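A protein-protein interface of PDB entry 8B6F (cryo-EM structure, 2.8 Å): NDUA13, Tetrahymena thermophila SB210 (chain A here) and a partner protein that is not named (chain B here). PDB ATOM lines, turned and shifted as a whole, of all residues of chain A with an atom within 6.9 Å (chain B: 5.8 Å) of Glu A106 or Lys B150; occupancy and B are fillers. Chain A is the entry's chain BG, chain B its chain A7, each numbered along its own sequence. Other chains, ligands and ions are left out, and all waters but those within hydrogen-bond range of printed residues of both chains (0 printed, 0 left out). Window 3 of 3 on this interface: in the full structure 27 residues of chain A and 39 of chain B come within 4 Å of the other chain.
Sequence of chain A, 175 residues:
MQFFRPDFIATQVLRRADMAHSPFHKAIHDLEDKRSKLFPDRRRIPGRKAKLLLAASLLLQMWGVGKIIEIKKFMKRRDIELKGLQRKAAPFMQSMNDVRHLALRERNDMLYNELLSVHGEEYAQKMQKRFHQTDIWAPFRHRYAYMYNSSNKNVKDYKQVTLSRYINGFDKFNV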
ATOM      1  N   ASP A  98      -7.134 -12.561  28.254  1.00  0.00           N
ATOM      2  CA  ASP A  98      -6.942 -13.763  27.451  1.00  0.00           C
ATOM      3  C   ASP A  98      -5.498 -14.242  27.495  1.00  0.00           C
ATOM      4  O   ASP A  98      -5.242 -15.447  27.597  1.00  0.00           O
ATOM      5  CB  ASP A  98      -7.369 -13.497  26.007  1.00  0.00           C
ATOM      6  CG  ASP A  98      -8.868 -13.347  25.862  1.00  0.00           C
ATOM      7  OD1 ASP A  98      -9.573 -13.373  26.891  1.00  0.00           O
ATOM      8  OD2 ASP A  98      -9.345 -13.210  24.716  1.00  0.00           O
ATOM      9  N   VAL A  99      -4.538 -13.319  27.428  1.00  0.00           N
ATOM     10  CA  VAL A  99      -3.135 -13.718  27.465  1.00  0.00           C
ATOM     11  C   VAL A  99      -2.803 -14.377  28.797  1.00  0.00           C
ATOM     12  O   VAL A  99      -2.128 -15.414  28.841  1.00  0.00           O
ATOM     13  CB  VAL A  99      -2.225 -12.509  27.183  1.00  0.00           C
ATOM     14  CG1 VAL A  99      -0.784 -12.828  27.532  1.00  0.00           C
ATOM     15  CG2 VAL A  99      -2.338 -12.095  25.730  1.00  0.00           C
ATOM     16  N   ARG A 100      -3.259 -13.789  29.903  1.00  0.00           N
ATOM     17  CA  ARG A 100      -3.002 -14.389  31.206  1.00  0.00           C
ATOM     18  C   ARG A 100      -3.663 -15.755  31.312  1.00  0.00           C
ATOM     19  O   ARG A 100      -3.064 -16.710  31.817  1.00  0.00           O
ATOM     20  CB  ARG A 100      -3.496 -13.467  32.318  1.00  0.00           C
ATOM     21  CG  ARG A 100      -2.753 -12.146  32.407  1.00  0.00           C
ATOM     22  CD  ARG A 100      -3.171 -11.384  33.650  1.00  0.00           C
ATOM     23  NE  ARG A 100      -2.431 -10.139  33.822  1.00  0.00           N
ATOM     24  CZ  ARG A 100      -2.842  -8.951  33.398  1.00  0.00           C
ATOM     25  NH1 ARG A 100      -3.986  -8.802  32.754  1.00  0.00           N
ATOM     26  NH2 ARG A 100      -2.090  -7.882  33.640  1.00  0.00           N
ATOM     27  N   HIS A 101      -4.904 -15.864  30.836  1.00  0.00           N
ATOM     28  CA  HIS A 101      -5.615 -17.136  30.883  1.00  0.00           C
ATOM     29  C   HIS A 101      -4.879 -18.205  30.088  1.00  0.00           C
ATOM     30  O   HIS A 101      -4.753 -19.349  30.537  1.00  0.00           O
ATOM     31  CB  HIS A 101      -7.034 -16.944  30.348  1.00  0.00           C
ATOM     32  CG  HIS A 101      -7.900 -18.158  30.465  1.00  0.00           C
ATOM     33  ND1 HIS A 101      -8.150 -18.996  29.402  1.00  0.00           N
ATOM     34  CD2 HIS A 101      -8.579 -18.670  31.517  1.00  0.00           C
ATOM     35  CE1 HIS A 101      -8.944 -19.975  29.794  1.00  0.00           C
ATOM     36  NE2 HIS A 101      -9.222 -19.801  31.072  1.00  0.00           N
ATOM     37  N   LEU A 102      -4.384 -17.849  28.901  1.00  0.00           N
ATOM     38  CA  LEU A 102      -3.656 -18.806  28.076  1.00  0.00           C
ATOM     39  C   LEU A 102      -2.310 -19.174  28.685  1.00  0.00           C
ATOM     40  O   LEU A 102      -1.855 -20.314  28.529  1.00  0.00           O
ATOM     41  CB  LEU A 102      -3.469 -18.243  26.668  1.00  0.00           C
ATOM     42  CG  LEU A 102      -4.762 -18.045  25.875  1.00  0.00           C
ATOM     43  CD1 LEU A 102      -4.481 -17.325  24.571  1.00  0.00           C
ATOM     44  CD2 LEU A 102      -5.447 -19.376  25.606  1.00  0.00           C
ATOM     45  N   ALA A 103      -1.656 -18.238  29.374  1.00  0.00           N
ATOM     46  CA  ALA A 103      -0.416 -18.571  30.065  1.00  0.00           C
ATOM     47  C   ALA A 103      -0.660 -19.610  31.151  1.00  0.00           C
ATOM     48  O   ALA A 103       0.101 -20.574  31.286  1.00  0.00           O
ATOM     49  CB  ALA A 103       0.211 -17.309  30.657  1.00  0.00           C
ATOM     50  N   LEU A 104      -1.713 -19.422  31.950  1.00  0.00           N
ATOM     51  CA  LEU A 104      -2.035 -20.413  32.971  1.00  0.00           C
ATOM     52  C   LEU A 104      -2.390 -21.751  32.337  1.00  0.00           C
ATOM     53  O   LEU A 104      -2.000 -22.810  32.842  1.00  0.00           O
ATOM     54  CB  LEU A 104      -3.179 -19.915  33.853  1.00  0.00           C
ATOM     55  CG  LEU A 104      -2.719 -19.140  35.089  1.00  0.00           C
ATOM     56  CD1 LEU A 104      -2.100 -17.819  34.685  1.00  0.00           C
ATOM     57  CD2 LEU A 104      -3.860 -18.916  36.062  1.00  0.00           C
ATOM     58  N   ARG A 105      -3.141 -21.724  31.232  1.00  0.00           N
ATOM     59  CA  ARG A 105      -3.487 -22.962  30.542  1.00  0.00           C
ATOM     60  C   ARG A 105      -2.247 -23.672  30.017  1.00  0.00           C
ATOM     61  O   ARG A 105      -2.150 -24.901  30.090  1.00  0.00           O
ATOM     62  CB  ARG A 105      -4.461 -22.674  29.399  1.00  0.00           C
ATOM     63  CG  ARG A 105      -5.910 -22.584  29.847  1.00  0.00           C
ATOM     64  CD  ARG A 105      -6.848 -22.282  28.689  1.00  0.00           C
ATOM     65  NE  ARG A 105      -6.739 -23.261  27.614  1.00  0.00           N
ATOM     66  CZ  ARG A 105      -7.484 -23.254  26.518  1.00  0.00           C
ATOM     67  NH1 ARG A 105      -8.412 -22.334  26.318  1.00  0.00           N
ATOM     68  NH2 ARG A 105      -7.294 -24.197  25.599  1.00  0.00           N
ATOM     69  N   GLU A 106      -1.284 -22.916  29.482  1.00  0.00           N
ATOM     70  CA  GLU A 106      -0.050 -23.531  29.006  1.00  0.00           C
ATOM     71  C   GLU A 106       0.720 -24.179  30.148  1.00  0.00           C
ATOM     72  O   GLU A 106       1.236 -25.292  30.003  1.00  0.00           O
ATOM     73  CB  GLU A 106       0.822 -22.494  28.301  1.00  0.00           C
ATOM     74  CG  GLU A 106       0.322 -22.110  26.918  1.00  0.00           C
ATOM     75  CD  GLU A 106       1.246 -21.138  26.218  1.00  0.00           C
ATOM     76  OE1 GLU A 106       2.176 -20.626  26.875  1.00  0.00           O
ATOM     77  OE2 GLU A 106       1.048 -20.889  25.010  1.00  0.00           O
ATOM     78  N   ARG A 107       0.811 -23.500  31.291  1.00  0.00           N
ATOM     79  CA  ARG A 107       1.480 -24.096  32.441  1.00  0.00           C
ATOM     80  C   ARG A 107       0.794 -25.394  32.847  1.00  0.00           C
ATOM     81  O   ARG A 107       1.454 -26.410  33.094  1.00  0.00           O
ATOM     82  CB  ARG A 107       1.503 -23.108  33.607  1.00  0.00           C
ATOM     83  CG  ARG A 107       2.225 -23.630  34.840  1.00  0.00           C
ATOM     84  CD  ARG A 107       2.033 -22.712  36.032  1.00  0.00           C
ATOM     85  NE  ARG A 107       0.628 -22.588  36.403  1.00  0.00           N
ATOM     86  CZ  ARG A 107      -0.035 -23.463  37.145  1.00  0.00           C
ATOM     87  NH1 ARG A 107       0.547 -24.554  37.613  1.00  0.00           N
ATOM     88  NH2 ARG A 107      -1.315 -23.238  37.426  1.00  0.00           N
ATOM     89  N   ASN A 108      -0.538 -25.377  32.922  1.00  0.00           N
ATOM     90  CA  ASN A 108      -1.270 -26.576  33.316  1.00  0.00           C
ATOM     91  C   ASN A 108      -1.089 -27.690  32.295  1.00  0.00           C
ATOM     92  O   ASN A 108      -0.964 -28.864  32.662  1.00  0.00           O
ATOM     93  CB  ASN A 108      -2.753 -26.253  33.499  1.00  0.00           C
ATOM     94  CG  ASN A 108      -3.044 -25.589  34.826  1.00  0.00           C
ATOM     95  OD1 ASN A 108      -2.377 -25.851  35.825  1.00  0.00           O
ATOM     96  ND2 ASN A 108      -4.048 -24.724  34.846  1.00  0.00           N
ATOM     97  N   ASP A 109      -1.078 -27.346  31.007  1.00  0.00           N
ATOM     98  CA  ASP A 109      -0.875 -28.364  29.983  1.00  0.00           C
ATOM     99  C   ASP A 109       0.503 -28.998  30.111  1.00  0.00           C
ATOM    100  O   ASP A 109       0.645 -30.220  29.995  1.00  0.00           O
ATOM    101  CB  ASP A 109      -1.059 -27.757  28.592  1.00  0.00           C
ATOM    102  CG  ASP A 109      -2.476 -27.272  28.351  1.00  0.00           C
ATOM    103  OD1 ASP A 109      -3.321 -27.428  29.256  1.00  0.00           O
ATOM    104  OD2 ASP A 109      -2.745 -26.735  27.255  1.00  0.00           O
ATOM    105  N   MET A 110       1.535 -28.186  30.345  1.00  0.00           N
ATOM    106  CA  MET A 110       2.874 -28.735  30.532  1.00  0.00           C
ATOM    107  C   MET A 110       2.918 -29.662  31.738  1.00  0.00           C
ATOM    108  O   MET A 110       3.488 -30.756  31.675  1.00  0.00           O
ATOM    109  CB  MET A 110       3.885 -27.600  30.694  1.00  0.00           C
ATOM    110  CG  MET A 110       4.180 -26.847  29.410  1.00  0.00           C
ATOM    111  SD  MET A 110       5.122 -25.335  29.692  1.00  0.00           S
ATOM    112  CE  MET A 110       6.529 -25.965  30.600  1.00  0.00           C
ATOM    113  N   LEU A 111       2.324 -29.235  32.853  1.00  0.00           N
ATOM    114  CA  LEU A 111       2.330 -30.068  34.051  1.00  0.00           C
ATOM    115  C   LEU A 111       1.591 -31.378  33.806  1.00  0.00           C
ATOM    116  O   LEU A 111       2.073 -32.452  34.183  1.00  0.00           O
ATOM    117  CB  LEU A 111       1.712 -29.306  35.223  1.00  0.00           C
ATOM    118  CG  LEU A 111       1.645 -30.059  36.556  1.00  0.00           C
ATOM    119  CD1 LEU A 111       1.958 -29.131  37.710  1.00  0.00           C
ATOM    120  CD2 LEU A 111       0.285 -30.699  36.758  1.00  0.00           C
ATOM    121  N   TYR A 112       0.421 -31.310  33.165  1.00  0.00           N
ATOM    122  CA  TYR A 112      -0.347 -32.521  32.897  1.00  0.00           C
ATOM    123  C   TYR A 112       0.417 -33.466  31.979  1.00  0.00           C
ATOM    124  O   TYR A 112       0.453 -34.679  32.217  1.00  0.00           O
ATOM    125  CB  TYR A 112      -1.700 -32.168  32.276  1.00  0.00           C
ATOM    126  CG  TYR A 112      -2.655 -31.425  33.188  1.00  0.00           C
ATOM    127  CD1 TYR A 112      -2.323 -31.142  34.507  1.00  0.00           C
ATOM    128  CD2 TYR A 112      -3.900 -31.019  32.727  1.00  0.00           C
ATOM    129  CE1 TYR A 112      -3.199 -30.471  35.337  1.00  0.00           C
ATOM    130  CE2 TYR A 112      -4.784 -30.347  33.549  1.00  0.00           C
ATOM    131  CZ  TYR A 112      -4.428 -30.076  34.853  1.00  0.00           C
ATOM    132  OH  TYR A 112      -5.305 -29.407  35.675  1.00  0.00           O
ATOM    133  N   ASN A 113       1.036 -32.932  30.926  1.00  0.00           N
ATOM    134  CA  ASN A 113       1.800 -33.782  30.021  1.00  0.00           C
ATOM    135  C   ASN A 113       2.952 -34.465  30.747  1.00  0.00           C
ATOM    136  O   ASN A 113       3.182 -35.665  30.568  1.00  0.00           O
ATOM    137  CB  ASN A 113       2.327 -32.959  28.845  1.00  0.00           C
ATOM    138  CG  ASN A 113       1.223 -32.497  27.917  1.00  0.00           C
ATOM    139  OD1 ASN A 113       0.205 -33.169  27.761  1.00  0.00           O
ATOM    140  ND2 ASN A 113       1.421 -31.342  27.290  1.00  0.00           N
ATOM    141  N   PRO B 146     -10.091 -18.376  23.883  1.00  0.00           N
ATOM    142  CA  PRO B 146      -9.008 -17.414  23.609  1.00  0.00           C
ATOM    143  C   PRO B 146      -7.841 -17.997  22.836  1.00  0.00           C
ATOM    144  O   PRO B 146      -7.040 -17.230  22.289  1.00  0.00           O
ATOM    145  CB  PRO B 146      -8.571 -16.965  25.012  1.00  0.00           C
ATOM    146  CG  PRO B 146      -9.712 -17.279  25.895  1.00  0.00           C
ATOM    147  CD  PRO B 146     -10.351 -18.502  25.327  1.00  0.00           C
ATOM    148  N   ILE B 147      -7.716 -19.322  22.763  1.00  0.00           N
ATOM    149  CA  ILE B 147      -6.582 -19.923  22.069  1.00  0.00           C
ATOM    150  C   ILE B 147      -6.605 -19.558  20.593  1.00  0.00           C
ATOM    151  O   ILE B 147      -5.550 -19.438  19.957  1.00  0.00           O
ATOM    152  CB  ILE B 147      -6.577 -21.451  22.282  1.00  0.00           C
ATOM    153  CG1 ILE B 147      -5.244 -22.057  21.839  1.00  0.00           C
ATOM    154  CG2 ILE B 147      -7.712 -22.109  21.511  1.00  0.00           C
ATOM    155  CD1 ILE B 147      -4.059 -21.645  22.692  1.00  0.00           C
ATOM    156  N   HIS B 148      -7.795 -19.374  20.022  1.00  0.00           N
ATOM    157  CA  HIS B 148      -7.905 -18.991  18.620  1.00  0.00           C
ATOM    158  C   HIS B 148      -7.553 -17.526  18.397  1.00  0.00           C
ATOM    159  O   HIS B 148      -7.018 -17.177  17.339  1.00  0.00           O
ATOM    160  CB  HIS B 148      -9.320 -19.269  18.108  1.00  0.00           C
ATOM    161  CG  HIS B 148      -9.733 -20.704  18.221  1.00  0.00           C
ATOM    162  ND1 HIS B 148      -9.910 -21.336  19.433  1.00  0.00           N
ATOM    163  CD2 HIS B 148     -10.002 -21.630  17.271  1.00  0.00           C
ATOM    164  CE1 HIS B 148     -10.271 -22.590  19.226  1.00  0.00           C
ATOM    165  NE2 HIS B 148     -10.335 -22.794  17.923  1.00  0.00           N
ATOM    166  N   CYS B 149      -7.845 -16.659  19.365  1.00  0.00           N
ATOM    167  CA  CYS B 149      -7.633 -15.225  19.228  1.00  0.00           C
ATOM    168  C   CYS B 149      -6.334 -14.760  19.873  1.00  0.00           C
ATOM    169  O   CYS B 149      -6.093 -13.551  19.952  1.00  0.00           O
ATOM    170  CB  CYS B 149      -8.812 -14.464  19.839  1.00  0.00           C
ATOM    171  SG  CYS B 149     -10.420 -15.230  19.543  1.00  0.00           S
ATOM    172  N   LYS B 150      -5.498 -15.689  20.340  1.00  0.00           N
ATOM    173  CA  LYS B 150      -4.240 -15.312  20.978  1.00  0.00           C
ATOM    174  C   LYS B 150      -3.405 -14.386  20.101  1.00  0.00           C
ATOM    175  O   LYS B 150      -2.848 -13.397  20.588  1.00  0.00           O
ATOM    176  CB  LYS B 150      -3.441 -16.567  21.327  1.00  0.00           C
ATOM    177  CG  LYS B 150      -2.148 -16.285  22.077  1.00  0.00           C
ATOM    178  CD  LYS B 150      -1.413 -17.570  22.418  1.00  0.00           C
ATOM    179  CE  LYS B 150      -0.113 -17.279  23.148  1.00  0.00           C
ATOM    180  NZ  LYS B 150       0.571 -18.527  23.584  1.00  0.00           N
ATOM    181  N   ALA B 151      -3.301 -14.688  18.805  1.00  0.00           N
ATOM    182  CA  ALA B 151      -2.437 -13.891  17.939  1.00  0.00           C
ATOM    183  C   ALA B 151      -2.947 -12.461  17.814  1.00  0.00           C
ATOM    184  O   ALA B 151      -2.174 -11.504  17.930  1.00  0.00           O
ATOM    185  CB  ALA B 151      -2.331 -14.545  16.562  1.00  0.00           C
ATOM    186  N   GLN B 152      -4.247 -12.295  17.568  1.00  0.00           N
ATOM    187  CA  GLN B 152      -4.811 -10.953  17.480  1.00  0.00           C
ATOM    188  C   GLN B 152      -4.679 -10.217  18.806  1.00  0.00           C
ATOM    189  O   GLN B 152      -4.416  -9.011  18.834  1.00  0.00           O
ATOM    190  CB  GLN B 152      -6.273 -11.016  17.042  1.00  0.00           C
ATOM    191  CG  GLN B 152      -6.472 -11.410  15.587  1.00  0.00           C
ATOM    192  CD  GLN B 152      -6.189 -12.873  15.327  1.00  0.00           C
ATOM    193  OE1 GLN B 152      -5.910 -13.636  16.249  1.00  0.00           O
ATOM    194  NE2 GLN B 152      -6.255 -13.271  14.062  1.00  0.00           N
ATOM    195  N   ALA B 153      -4.847 -10.933  19.920  1.00  0.00           N
ATOM    196  CA  ALA B 153      -4.687 -10.312  21.229  1.00  0.00           C
ATOM    197  C   ALA B 153      -3.262  -9.817  21.431  1.00  0.00           C
ATOM    198  O   ALA B 153      -3.047  -8.720  21.958  1.00  0.00           O
ATOM    199  CB  ALA B 153      -5.075 -11.301  22.328  1.00  0.00           C
ATOM    200  N   LYS B 154      -2.273 -10.609  21.015  1.00  0.00           N
ATOM    201  CA  LYS B 154      -0.886 -10.175  21.134  1.00  0.00           C
ATOM    202  C   LYS B 154      -0.624  -8.937  20.286  1.00  0.00           C
ATOM    203  O   LYS B 154       0.055  -8.005  20.729  1.00  0.00           O
ATOM    204  CB  LYS B 154       0.056 -11.309  20.735  1.00  0.00           C
ATOM    205  CG  LYS B 154       0.278 -12.331  21.835  1.00  0.00           C
ATOM    206  CD  LYS B 154       1.243 -13.415  21.391  1.00  0.00           C
ATOM    207  CE  LYS B 154       1.666 -14.290  22.556  1.00  0.00           C
ATOM    208  NZ  LYS B 154       2.490 -13.544  23.546  1.00  0.00           N
ATOM    209  N   GLU B 155      -1.153  -8.910  19.061  1.00  0.00           N
ATOM    210  CA  GLU B 155      -0.992  -7.730  18.219  1.00  0.00           C
ATOM    211  C   GLU B 155      -1.624  -6.505  18.867  1.00  0.00           C
ATOM    212  O   GLU B 155      -1.027  -5.422  18.879  1.00  0.00           O
ATOM    213  CB  GLU B 155      -1.608  -7.980  16.843  1.00  0.00           C
ATOM    214  CG  GLU B 155      -0.925  -9.076  16.043  1.00  0.00           C
ATOM    215  CD  GLU B 155       0.451  -8.674  15.551  1.00  0.00           C
ATOM    216  OE1 GLU B 155       0.875  -7.533  15.828  1.00  0.00           O
ATOM    217  OE2 GLU B 155       1.108  -9.499  14.882  1.00  0.00           O
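The side-chain carboxylate (OE2) of Glu A106 is in salt-bridge range of the side-chain amino group (NZ) of Lys B150, at 2.8 Å.
CB of Pro B146 touches CG of Asp A98, at 3.7 Å. Leu A102 touches Pro B146. Leu A102 touches Ile B147. Leu A102 touches Lys B150.
Glu A106 touches one residue of chain B. Of chain A, only Leu A102 and Glu A106 come within 4 Å of Lys B150. Of the printed residues of chain B, Asp A98 touches Pro B146. Printed residues of chain B within 4 Å of Leu A102: Pro B146 (3.4 Å), Ile B147 (3.6 Å) and Lys B150 (3.5 Å). Printed residues of chain A within 4 Å of Ile B147: Leu A102. Tyr A112 touches none of the printed residues of chain B. His B148 touches none of the printed residues of chain A. The nearest printed residue of chain A that does not touch Ile B147 is Arg A105 (4.4 Å).
Hydrophobic or aromatic side chains of chain B within 4 Å of the printed part of chain A: Pro B146 and Ile B147. Of the 16 printed residues of chain A, 3 touch a printed residue of chain B. Hydrophobic or aromatic side chains of chain A within 4 Å of the printed part of chain B: Leu A102. Among the printed residues, 5 pairs touch across the chains.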
